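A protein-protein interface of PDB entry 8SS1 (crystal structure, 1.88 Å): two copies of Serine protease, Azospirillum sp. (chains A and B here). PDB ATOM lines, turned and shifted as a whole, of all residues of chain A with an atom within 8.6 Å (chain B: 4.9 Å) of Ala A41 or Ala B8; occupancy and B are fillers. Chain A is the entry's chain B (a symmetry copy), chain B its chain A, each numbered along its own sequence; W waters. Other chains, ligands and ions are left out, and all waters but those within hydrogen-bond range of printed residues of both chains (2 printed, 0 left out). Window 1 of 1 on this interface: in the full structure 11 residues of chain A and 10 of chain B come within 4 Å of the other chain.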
ATOM      1  N   PRO A  34     -24.888 -20.262   7.636  1.00  0.00           N
ATOM      2  CA  PRO A  34     -23.926 -19.466   6.856  1.00  0.00           C
ATOM      3  C   PRO A  34     -24.409 -19.158   5.453  1.00  0.00           C
ATOM      4  O   PRO A  34     -24.234 -18.033   4.977  1.00  0.00           O
ATOM      5  CB  PRO A  34     -22.673 -20.353   6.843  1.00  0.00           C
ATOM      6  CG  PRO A  34     -22.767 -21.127   8.104  1.00  0.00           C
ATOM      7  CD  PRO A  34     -24.230 -21.406   8.297  1.00  0.00           C
ATOM      8  N   GLN A  35     -25.035 -20.128   4.782  1.00  0.00           N
ATOM      9  CA  GLN A  35     -25.454 -19.914   3.401  1.00  0.00           C
ATOM     10  C   GLN A  35     -26.635 -18.956   3.318  1.00  0.00           C
ATOM     11  O   GLN A  35     -26.669 -18.085   2.442  1.00  0.00           O
ATOM     12  CB  GLN A  35     -25.795 -21.251   2.745  1.00  0.00           C
ATOM     13  CG  GLN A  35     -24.574 -22.161   2.571  1.00  0.00           C
ATOM     14  CD  GLN A  35     -24.937 -23.570   2.131  1.00  0.00           C
ATOM     15  OE1 GLN A  35     -26.014 -24.073   2.448  1.00  0.00           O
ATOM     16  NE2 GLN A  35     -24.032 -24.219   1.397  1.00  0.00           N
ATOM     17  N   LEU A  36     -27.612 -19.099   4.214  1.00  0.00           N
ATOM     18  CA  LEU A  36     -28.743 -18.174   4.228  1.00  0.00           C
ATOM     19  C   LEU A  36     -28.281 -16.745   4.467  1.00  0.00           C
ATOM     20  O   LEU A  36     -28.701 -15.818   3.766  1.00  0.00           O
ATOM     21  CB  LEU A  36     -29.745 -18.572   5.313  1.00  0.00           C
ATOM     22  CG  LEU A  36     -30.554 -19.857   5.218  1.00  0.00           C
ATOM     23  CD1 LEU A  36     -31.384 -19.963   6.476  1.00  0.00           C
ATOM     24  CD2 LEU A  36     -31.446 -19.844   3.995  1.00  0.00           C
ATOM     25  N   GLU A  37     -27.436 -16.547   5.480  1.00  0.00           N
ATOM     26  CA  GLU A  37     -26.961 -15.206   5.797  1.00  0.00           C
ATOM     27  C   GLU A  37     -26.145 -14.626   4.650  1.00  0.00           C
ATOM     28  O   GLU A  37     -26.294 -13.448   4.307  1.00  0.00           O
ATOM     29  CB  GLU A  37     -26.142 -15.231   7.092  1.00  0.00           C
ATOM     30  CG  GLU A  37     -26.924 -15.711   8.322  1.00  0.00           C
ATOM     31  CD  GLU A  37     -26.085 -15.707   9.589  1.00  0.00           C
ATOM     32  OE1 GLU A  37     -24.963 -15.156   9.546  1.00  0.00           O
ATOM     33  OE2 GLU A  37     -26.539 -16.261  10.619  1.00  0.00           O
ATOM     34  N   ALA A  38     -25.291 -15.444   4.028  1.00  0.00           N
ATOM     35  CA  ALA A  38     -24.475 -14.957   2.921  1.00  0.00           C
ATOM     36  C   ALA A  38     -25.334 -14.576   1.719  1.00  0.00           C
ATOM     37  O   ALA A  38     -25.095 -13.545   1.081  1.00  0.00           O
ATOM     38  CB  ALA A  38     -23.437 -16.014   2.535  1.00  0.00           C
ATOM     39  N   ASP A  39     -26.339 -15.395   1.392  1.00  0.00           N
ATOM     40  CA  ASP A  39     -27.243 -15.064   0.291  1.00  0.00           C
ATOM     41  C   ASP A  39     -28.015 -13.777   0.563  1.00  0.00           C
ATOM     42  O   ASP A  39     -28.275 -12.996  -0.362  1.00  0.00           O
ATOM     43  CB  ASP A  39     -28.227 -16.205   0.041  1.00  0.00           C
ATOM     44  CG  ASP A  39     -27.565 -17.449  -0.503  1.00  0.00           C
ATOM     45  OD1 ASP A  39     -26.360 -17.407  -0.837  1.00  0.00           O
ATOM     46  OD2 ASP A  39     -28.268 -18.477  -0.597  1.00  0.00           O
ATOM     47  N   VAL A  40     -28.419 -13.545   1.813  1.00  0.00           N
ATOM     48  CA  VAL A  40     -29.117 -12.298   2.116  1.00  0.00           C
ATOM     49  C   VAL A  40     -28.161 -11.118   1.998  1.00  0.00           C
ATOM     50  O   VAL A  40     -28.541 -10.037   1.534  1.00  0.00           O
ATOM     51  CB  VAL A  40     -29.782 -12.368   3.504  1.00  0.00           C
ATOM     52  CG1 VAL A  40     -30.302 -10.993   3.926  1.00  0.00           C
ATOM     53  CG2 VAL A  40     -30.927 -13.362   3.483  1.00  0.00           C
ATOM     54  N   ALA A  41     -26.897 -11.313   2.385  1.00  0.00           N
ATOM     55  CA  ALA A  41     -25.910 -10.249   2.235  1.00  0.00           C
ATOM     56  C   ALA A  41     -25.577 -10.000   0.768  1.00  0.00           C
ATOM     57  O   ALA A  41     -25.455  -8.848   0.342  1.00  0.00           O
ATOM     58  CB  ALA A  41     -24.642 -10.583   3.019  1.00  0.00           C
ATOM     59  N   LEU A  42     -25.440 -11.065  -0.021  1.00  0.00           N
ATOM     60  CA  LEU A  42     -25.008 -10.905  -1.406  1.00  0.00           C
ATOM     61  C   LEU A  42     -26.117 -10.373  -2.307  1.00  0.00           C
ATOM     62  O   LEU A  42     -25.825  -9.711  -3.309  1.00  0.00           O
ATOM     63  CB  LEU A  42     -24.468 -12.230  -1.947  1.00  0.00           C
ATOM     64  CG  LEU A  42     -23.168 -12.706  -1.290  1.00  0.00           C
ATOM     65  CD1 LEU A  42     -22.847 -14.134  -1.701  1.00  0.00           C
ATOM     66  CD2 LEU A  42     -21.999 -11.779  -1.611  1.00  0.00           C
ATOM     67  N   LYS A  43     -27.383 -10.622  -1.970  1.00  0.00           N
ATOM     68  CA  LYS A  43     -28.488 -10.163  -2.800  1.00  0.00           C
ATOM     69  C   LYS A  43     -29.131  -8.890  -2.266  1.00  0.00           C
ATOM     70  O   LYS A  43     -30.189  -8.486  -2.759  1.00  0.00           O
ATOM     71  CB  LYS A  43     -29.528 -11.273  -2.958  1.00  0.00           C
ATOM     72  CG  LYS A  43     -28.925 -12.566  -3.500  1.00  0.00           C
ATOM     73  CD  LYS A  43     -29.779 -13.190  -4.593  1.00  0.00           C
ATOM     74  CE  LYS A  43     -29.077 -14.391  -5.215  1.00  0.00           C
ATOM     75  NZ  LYS A  43     -29.863 -14.970  -6.341  1.00  0.00           N
ATOM     76  N   ALA A  44     -28.501  -8.238  -1.295  1.00  0.00           N
ATOM     77  CA  ALA A  44     -28.996  -6.980  -0.750  1.00  0.00           C
ATOM     78  C   ALA A  44     -29.100  -5.908  -1.834  1.00  0.00           C
ATOM     79  O   ALA A  44     -29.961  -5.028  -1.767  1.00  0.00           O
ATOM     80  CB  ALA A  44     -28.095  -6.506   0.382  1.00  0.00           C
ATOM     81  N   LEU A  53     -33.111  -6.060   8.439  1.00  0.00           N
ATOM     82  CA  LEU A  53     -32.220  -7.171   8.112  1.00  0.00           C
ATOM     83  C   LEU A  53     -32.530  -8.424   8.926  1.00  0.00           C
ATOM     84  O   LEU A  53     -32.569  -9.534   8.385  1.00  0.00           O
ATOM     85  CB  LEU A  53     -30.773  -6.735   8.333  1.00  0.00           C
ATOM     86  CG  LEU A  53     -29.704  -7.822   8.281  1.00  0.00           C
ATOM     87  CD1 LEU A  53     -29.707  -8.506   6.925  1.00  0.00           C
ATOM     88  CD2 LEU A  53     -28.345  -7.221   8.599  1.00  0.00           C
ATOM     89  N   GLU A  54     -32.765  -8.269  10.229  1.00  0.00           N
ATOM     90  CA  GLU A  54     -32.996  -9.441  11.067  1.00  0.00           C
ATOM     91  C   GLU A  54     -34.297 -10.137  10.691  1.00  0.00           C
ATOM     92  O   GLU A  54     -34.377 -11.371  10.704  1.00  0.00           O
ATOM     93  CB  GLU A  54     -32.990  -9.042  12.539  1.00  0.00           C
ATOM     94  CG  GLU A  54     -32.808 -10.208  13.479  1.00  0.00           C
ATOM     95  CD  GLU A  54     -32.640  -9.765  14.913  1.00  0.00           C
ATOM     96  OE1 GLU A  54     -32.943  -8.592  15.216  1.00  0.00           O
ATOM     97  OE2 GLU A  54     -32.199 -10.586  15.738  1.00  0.00           O
ATOM     98  N   GLN A  56     -35.495 -10.136   7.628  1.00  0.00           N
ATOM     99  CA  GLN A  56     -35.215 -10.800   6.360  1.00  0.00           C
ATOM    100  C   GLN A  56     -34.600 -12.174   6.586  1.00  0.00           C
ATOM    101  O   GLN A  56     -34.950 -13.139   5.897  1.00  0.00           O
ATOM    102  CB  GLN A  56     -34.273  -9.950   5.501  1.00  0.00           C
ATOM    103  CG  GLN A  56     -34.867  -8.661   4.939  1.00  0.00           C
ATOM    104  CD  GLN A  56     -33.945  -8.019   3.916  1.00  0.00           C
ATOM    105  OE1 GLN A  56     -33.357  -8.710   3.085  1.00  0.00           O
ATOM    106  NE2 GLN A  56     -33.800  -6.698   3.982  1.00  0.00           N
ATOM    107  N   LEU A  57     -33.674 -12.277   7.542  1.00  0.00           N
ATOM    108  CA  LEU A  57     -33.026 -13.556   7.820  1.00  0.00           C
ATOM    109  C   LEU A  57     -34.025 -14.572   8.354  1.00  0.00           C
ATOM    110  O   LEU A  57     -34.061 -15.723   7.902  1.00  0.00           O
ATOM    111  CB  LEU A  57     -31.881 -13.351   8.811  1.00  0.00           C
ATOM    112  CG  LEU A  57     -30.703 -12.546   8.270  1.00  0.00           C
ATOM    113  CD1 LEU A  57     -29.832 -12.091   9.415  1.00  0.00           C
ATOM    114  CD2 LEU A  57     -29.904 -13.387   7.280  1.00  0.00           C
ATOM    115  N   GLU A  60     -36.283 -15.556   5.431  1.00  0.00           N
ATOM    116  CA  GLU A  60     -35.620 -16.486   4.520  1.00  0.00           C
ATOM    117  C   GLU A  60     -35.512 -17.878   5.132  1.00  0.00           C
ATOM    118  O   GLU A  60     -35.717 -18.881   4.440  1.00  0.00           O
ATOM    119  CB  GLU A  60     -34.237 -15.951   4.147  1.00  0.00           C
ATOM    120  CG  GLU A  60     -33.624 -16.590   2.908  1.00  0.00           C
ATOM    121  CD  GLU A  60     -34.436 -16.308   1.642  1.00  0.00           C
ATOM    122  OE1 GLU A  60     -35.119 -15.264   1.582  1.00  0.00           O
ATOM    123  OE2 GLU A  60     -34.392 -17.140   0.719  1.00  0.00           O
ATOM    124  N   GLU B   4     -21.480 -11.607   8.033  1.00  0.00           N
ATOM    125  CA  GLU B   4     -22.561 -11.595   7.056  1.00  0.00           C
ATOM    126  C   GLU B   4     -23.610 -10.543   7.404  1.00  0.00           C
ATOM    127  O   GLU B   4     -24.177  -9.913   6.508  1.00  0.00           O
ATOM    128  CB  GLU B   4     -23.206 -12.979   6.964  1.00  0.00           C
ATOM    129  CG  GLU B   4     -22.435 -13.988   6.118  1.00  0.00           C
ATOM    130  CD  GLU B   4     -21.235 -14.576   6.841  1.00  0.00           C
ATOM    131  OE1 GLU B   4     -21.107 -14.371   8.067  1.00  0.00           O
ATOM    132  OE2 GLU B   4     -20.416 -15.248   6.182  1.00  0.00           O
ATOM    133  N   ARG B   5     -23.886 -10.347   8.697  1.00  0.00           N
ATOM    134  CA  ARG B   5     -24.837  -9.316   9.112  1.00  0.00           C
ATOM    135  C   ARG B   5     -24.345  -7.928   8.720  1.00  0.00           C
ATOM    136  O   ARG B   5     -25.094  -7.130   8.147  1.00  0.00           O
ATOM    137  CB  ARG B   5     -25.071  -9.379  10.626  1.00  0.00           C
ATOM    138  CG  ARG B   5     -25.753 -10.636  11.125  1.00  0.00           C
ATOM    139  CD  ARG B   5     -27.271 -10.518  11.086  1.00  0.00           C
ATOM    140  NE  ARG B   5     -27.825  -9.609  12.083  1.00  0.00           N
ATOM    141  CZ  ARG B   5     -28.317  -9.983  13.257  1.00  0.00           C
ATOM    142  NH1 ARG B   5     -28.276 -11.245  13.657  1.00  0.00           N
ATOM    143  NH2 ARG B   5     -28.871  -9.069  14.049  1.00  0.00           N
ATOM    144  N   LEU B   6     -23.082  -7.626   9.030  1.00  0.00           N
ATOM    145  CA  LEU B   6     -22.517  -6.323   8.699  1.00  0.00           C
ATOM    146  C   LEU B   6     -22.505  -6.095   7.191  1.00  0.00           C
ATOM    147  O   LEU B   6     -22.898  -5.027   6.713  1.00  0.00           O
ATOM    148  CB  LEU B   6     -21.107  -6.205   9.279  1.00  0.00           C
ATOM    149  CG  LEU B   6     -20.344  -4.908   8.998  1.00  0.00           C
ATOM    150  CD1 LEU B   6     -21.121  -3.708   9.518  1.00  0.00           C
ATOM    151  CD2 LEU B   6     -18.960  -4.960   9.626  1.00  0.00           C
ATOM    152  N   ALA B   7     -22.053  -7.093   6.423  1.00  0.00           N
ATOM    153  CA  ALA B   7     -21.981  -6.949   4.971  1.00  0.00           C
ATOM    154  C   ALA B   7     -23.361  -6.731   4.363  1.00  0.00           C
ATOM    155  O   ALA B   7     -23.514  -5.958   3.407  1.00  0.00           O
ATOM    156  CB  ALA B   7     -21.312  -8.179   4.354  1.00  0.00           C
ATOM    157  N   ALA B   8     -24.380  -7.402   4.907  1.00  0.00           N
ATOM    158  CA  ALA B   8     -25.745  -7.217   4.428  1.00  0.00           C
ATOM    159  C   ALA B   8     -26.253  -5.816   4.733  1.00  0.00           C
ATOM    160  O   ALA B   8     -26.978  -5.221   3.927  1.00  0.00           O
ATOM    161  CB  ALA B   8     -26.669  -8.259   5.058  1.00  0.00           C
ATOM    162  N   TRP B   9     -25.874  -5.271   5.889  1.00  0.00           N
ATOM    163  CA  TRP B   9     -26.452  -4.015   6.355  1.00  0.00           C
ATOM    164  C   TRP B   9     -25.865  -2.809   5.638  1.00  0.00           C
ATOM    165  O   TRP B   9     -26.590  -1.857   5.321  1.00  0.00           O
ATOM    166  CB  TRP B   9     -26.243  -3.872   7.860  1.00  0.00           C
ATOM    167  CG  TRP B   9     -26.770  -2.586   8.417  1.00  0.00           C
ATOM    168  CD1 TRP B   9     -28.039  -2.346   8.863  1.00  0.00           C
ATOM    169  CD2 TRP B   9     -26.042  -1.366   8.596  1.00  0.00           C
ATOM    170  NE1 TRP B   9     -28.143  -1.049   9.306  1.00  0.00           N
ATOM    171  CE2 TRP B   9     -26.932  -0.426   9.150  1.00  0.00           C
ATOM    172  CE3 TRP B   9     -24.724  -0.974   8.335  1.00  0.00           C
ATOM    173  CZ2 TRP B   9     -26.547   0.881   9.454  1.00  0.00           C
ATOM    174  CZ3 TRP B   9     -24.342   0.322   8.639  1.00  0.00           C
ATOM    175  CH2 TRP B   9     -25.251   1.234   9.192  1.00  0.00           C
ATOM    176  N   THR B  10     -24.561  -2.817   5.392  1.00  0.00           N
ATOM    177  CA  THR B  10     -23.907  -1.626   4.878  1.00  0.00           C
ATOM    178  C   THR B  10     -24.373  -1.331   3.456  1.00  0.00           C
ATOM    179  O   THR B  10     -24.655  -2.240   2.669  1.00  0.00           O
ATOM    180  CB  THR B  10     -22.383  -1.790   4.927  1.00  0.00           C
ATOM    181  OG1 THR B  10     -21.754  -0.567   4.524  1.00  0.00           O
ATOM    182  CG2 THR B  10     -21.927  -2.912   4.016  1.00  0.00           C
ATOM    183  N   ARG B  55     -20.612  -6.486  -3.759  1.00  0.00           N
ATOM    184  CA  ARG B  55     -21.219  -7.179  -2.626  1.00  0.00           C
ATOM    185  C   ARG B  55     -20.352  -8.353  -2.177  1.00  0.00           C
ATOM    186  O   ARG B  55     -20.255  -8.640  -0.978  1.00  0.00           O
ATOM    187  CB  ARG B  55     -22.623  -7.647  -3.014  1.00  0.00           C
ATOM    188  CG  ARG B  55     -23.621  -7.703  -1.875  1.00  0.00           C
ATOM    189  CD  ARG B  55     -24.530  -6.479  -1.844  1.00  0.00           C
ATOM    190  NE  ARG B  55     -23.905  -5.365  -1.142  1.00  0.00           N
ATOM    191  CZ  ARG B  55     -23.858  -5.248   0.177  1.00  0.00           C
ATOM    192  NH1 ARG B  55     -24.403  -6.156   0.971  1.00  0.00           N
ATOM    193  NH2 ARG B  55     -23.240  -4.198   0.713  1.00  0.00           N
ATOM    194  N   LEU B  59     -18.473  -8.601   1.529  1.00  0.00           N
ATOM    195  CA  LEU B  59     -18.615  -9.796   2.354  1.00  0.00           C
ATOM    196  C   LEU B  59     -17.255 -10.405   2.676  1.00  0.00           C
ATOM    197  O   LEU B  59     -16.994 -10.786   3.824  1.00  0.00           O
ATOM    198  CB  LEU B  59     -19.513 -10.822   1.661  1.00  0.00           C
ATOM    199  CG  LEU B  59     -19.734 -12.135   2.430  1.00  0.00           C
ATOM    200  CD1 LEU B  59     -20.320 -11.886   3.820  1.00  0.00           C
ATOM    201  CD2 LEU B  59     -20.611 -13.106   1.643  1.00  0.00           C
HETATM  202  O   HOH W   1     -29.734 -11.306  16.518  1.00  0.00           O
HETATM  203  O   HOH W   2     -26.812 -11.347   6.550  1.00  0.00           O
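The guanidinium group (NH1) of Arg B55 lies within hydrogen-bond range of the backbone carbonyl oxygen (O) of Ala B7 (2.6 Å).
NH2 of Arg B55 lies within hydrogen-bond range of O of Thr B10, at 3.1 Å.
Printed residues of chain A that touch a printed residue of chain B: Glu A37, Ala A38, Ala A41, Leu A42, Ala A44, Leu A53, Glu A54 and Leu A57.
Hydrophobic or aromatic side chains of chain A within 4 Å of the printed part of chain B: Ala A41, Leu A42, Ala A44, Leu A53 and Leu A57.
Hydrophobic or aromatic side chains of chain B within 4 Å of the printed part of chain A: Ala B8 and Leu B59.
Among the printed residues, 13 pairs touch across the chains.
Among the printed residues, no Asp or Glu carboxylate lies within 4 Å of a Lys or Arg side-chain nitrogen of the other chain.
No position is printed for both chains.
Water W1 lies within hydrogen-bond range of the side-chain carboxylate (OE2) of Glu A54 (2.7 Å) and the guanidinium group (NH1) of Arg B5 (3.2 Å).
Water W2 lies within hydrogen-bond range of O of Glu B4 (3.0 Å) and O of Glu A37 (3.1 Å).
The guanidinium group (NH1) of Arg B55 sits at hydrogen-bond distance from the backbone carbonyl oxygen (O) of Ala A41 (3.0 Å).
Of chain B, only Glu B4, Ala B8 and Arg B55 come within 4 Å of Ala A41.
Of chain A, only Ala A41, Ala A44 and Leu A53 come within 4 Å of Ala B8.
No residue of chain A comes within 4 Å of Ala B7.
Of the printed residues of chain A, Arg B5 touches Leu A53, Glu A54 and Leu A57.
Of the printed residues of chain B, Leu A57 touches Arg B5.
Printed residues of chain A within 4 Å of Arg B55: Ala A41, Leu A42 and Ala A44.
Of the printed residues of chain B, Glu A54 touches Arg B5 (3.9 Å).
Of the printed residues of chain B, Leu A42 touches Arg B55 (3.3 Å) and Leu B59 (3.8 Å).
Lys A43 touches none of the printed residues of chain B.
Asp A39 touches none of the printed residues of chain B.
The nearest residue of chain A that does not touch Ala B8 is Val A40 (4.4 Å).
The nearest printed residue of chain A that does not touch Arg B55 is Lys A43 (4.8 Å).
Among the printed residues, merely in contact across the chains: Glu A37 with Glu B4 (3.7 Å), Ala A38 with Glu B4 (3.8 Å), Ala A41 with Glu B4 (3.6 Å), Ala A41 with Ala B8 (3.5 Å), Leu A42 with Arg B55 (3.3 Å), Leu A42 with Leu B59 (3.8 Å), Ala A44 with Ala B8 (3.9 Å), Ala A44 with Arg B55 (3.8 Å), Leu A53 with Arg B5 (3.3 Å), Leu A53 with Ala B8 (3.6 Å), Glu A54 with Arg B5 (3.9 Å) and Leu A57 with Arg B5 (3.4 Å).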
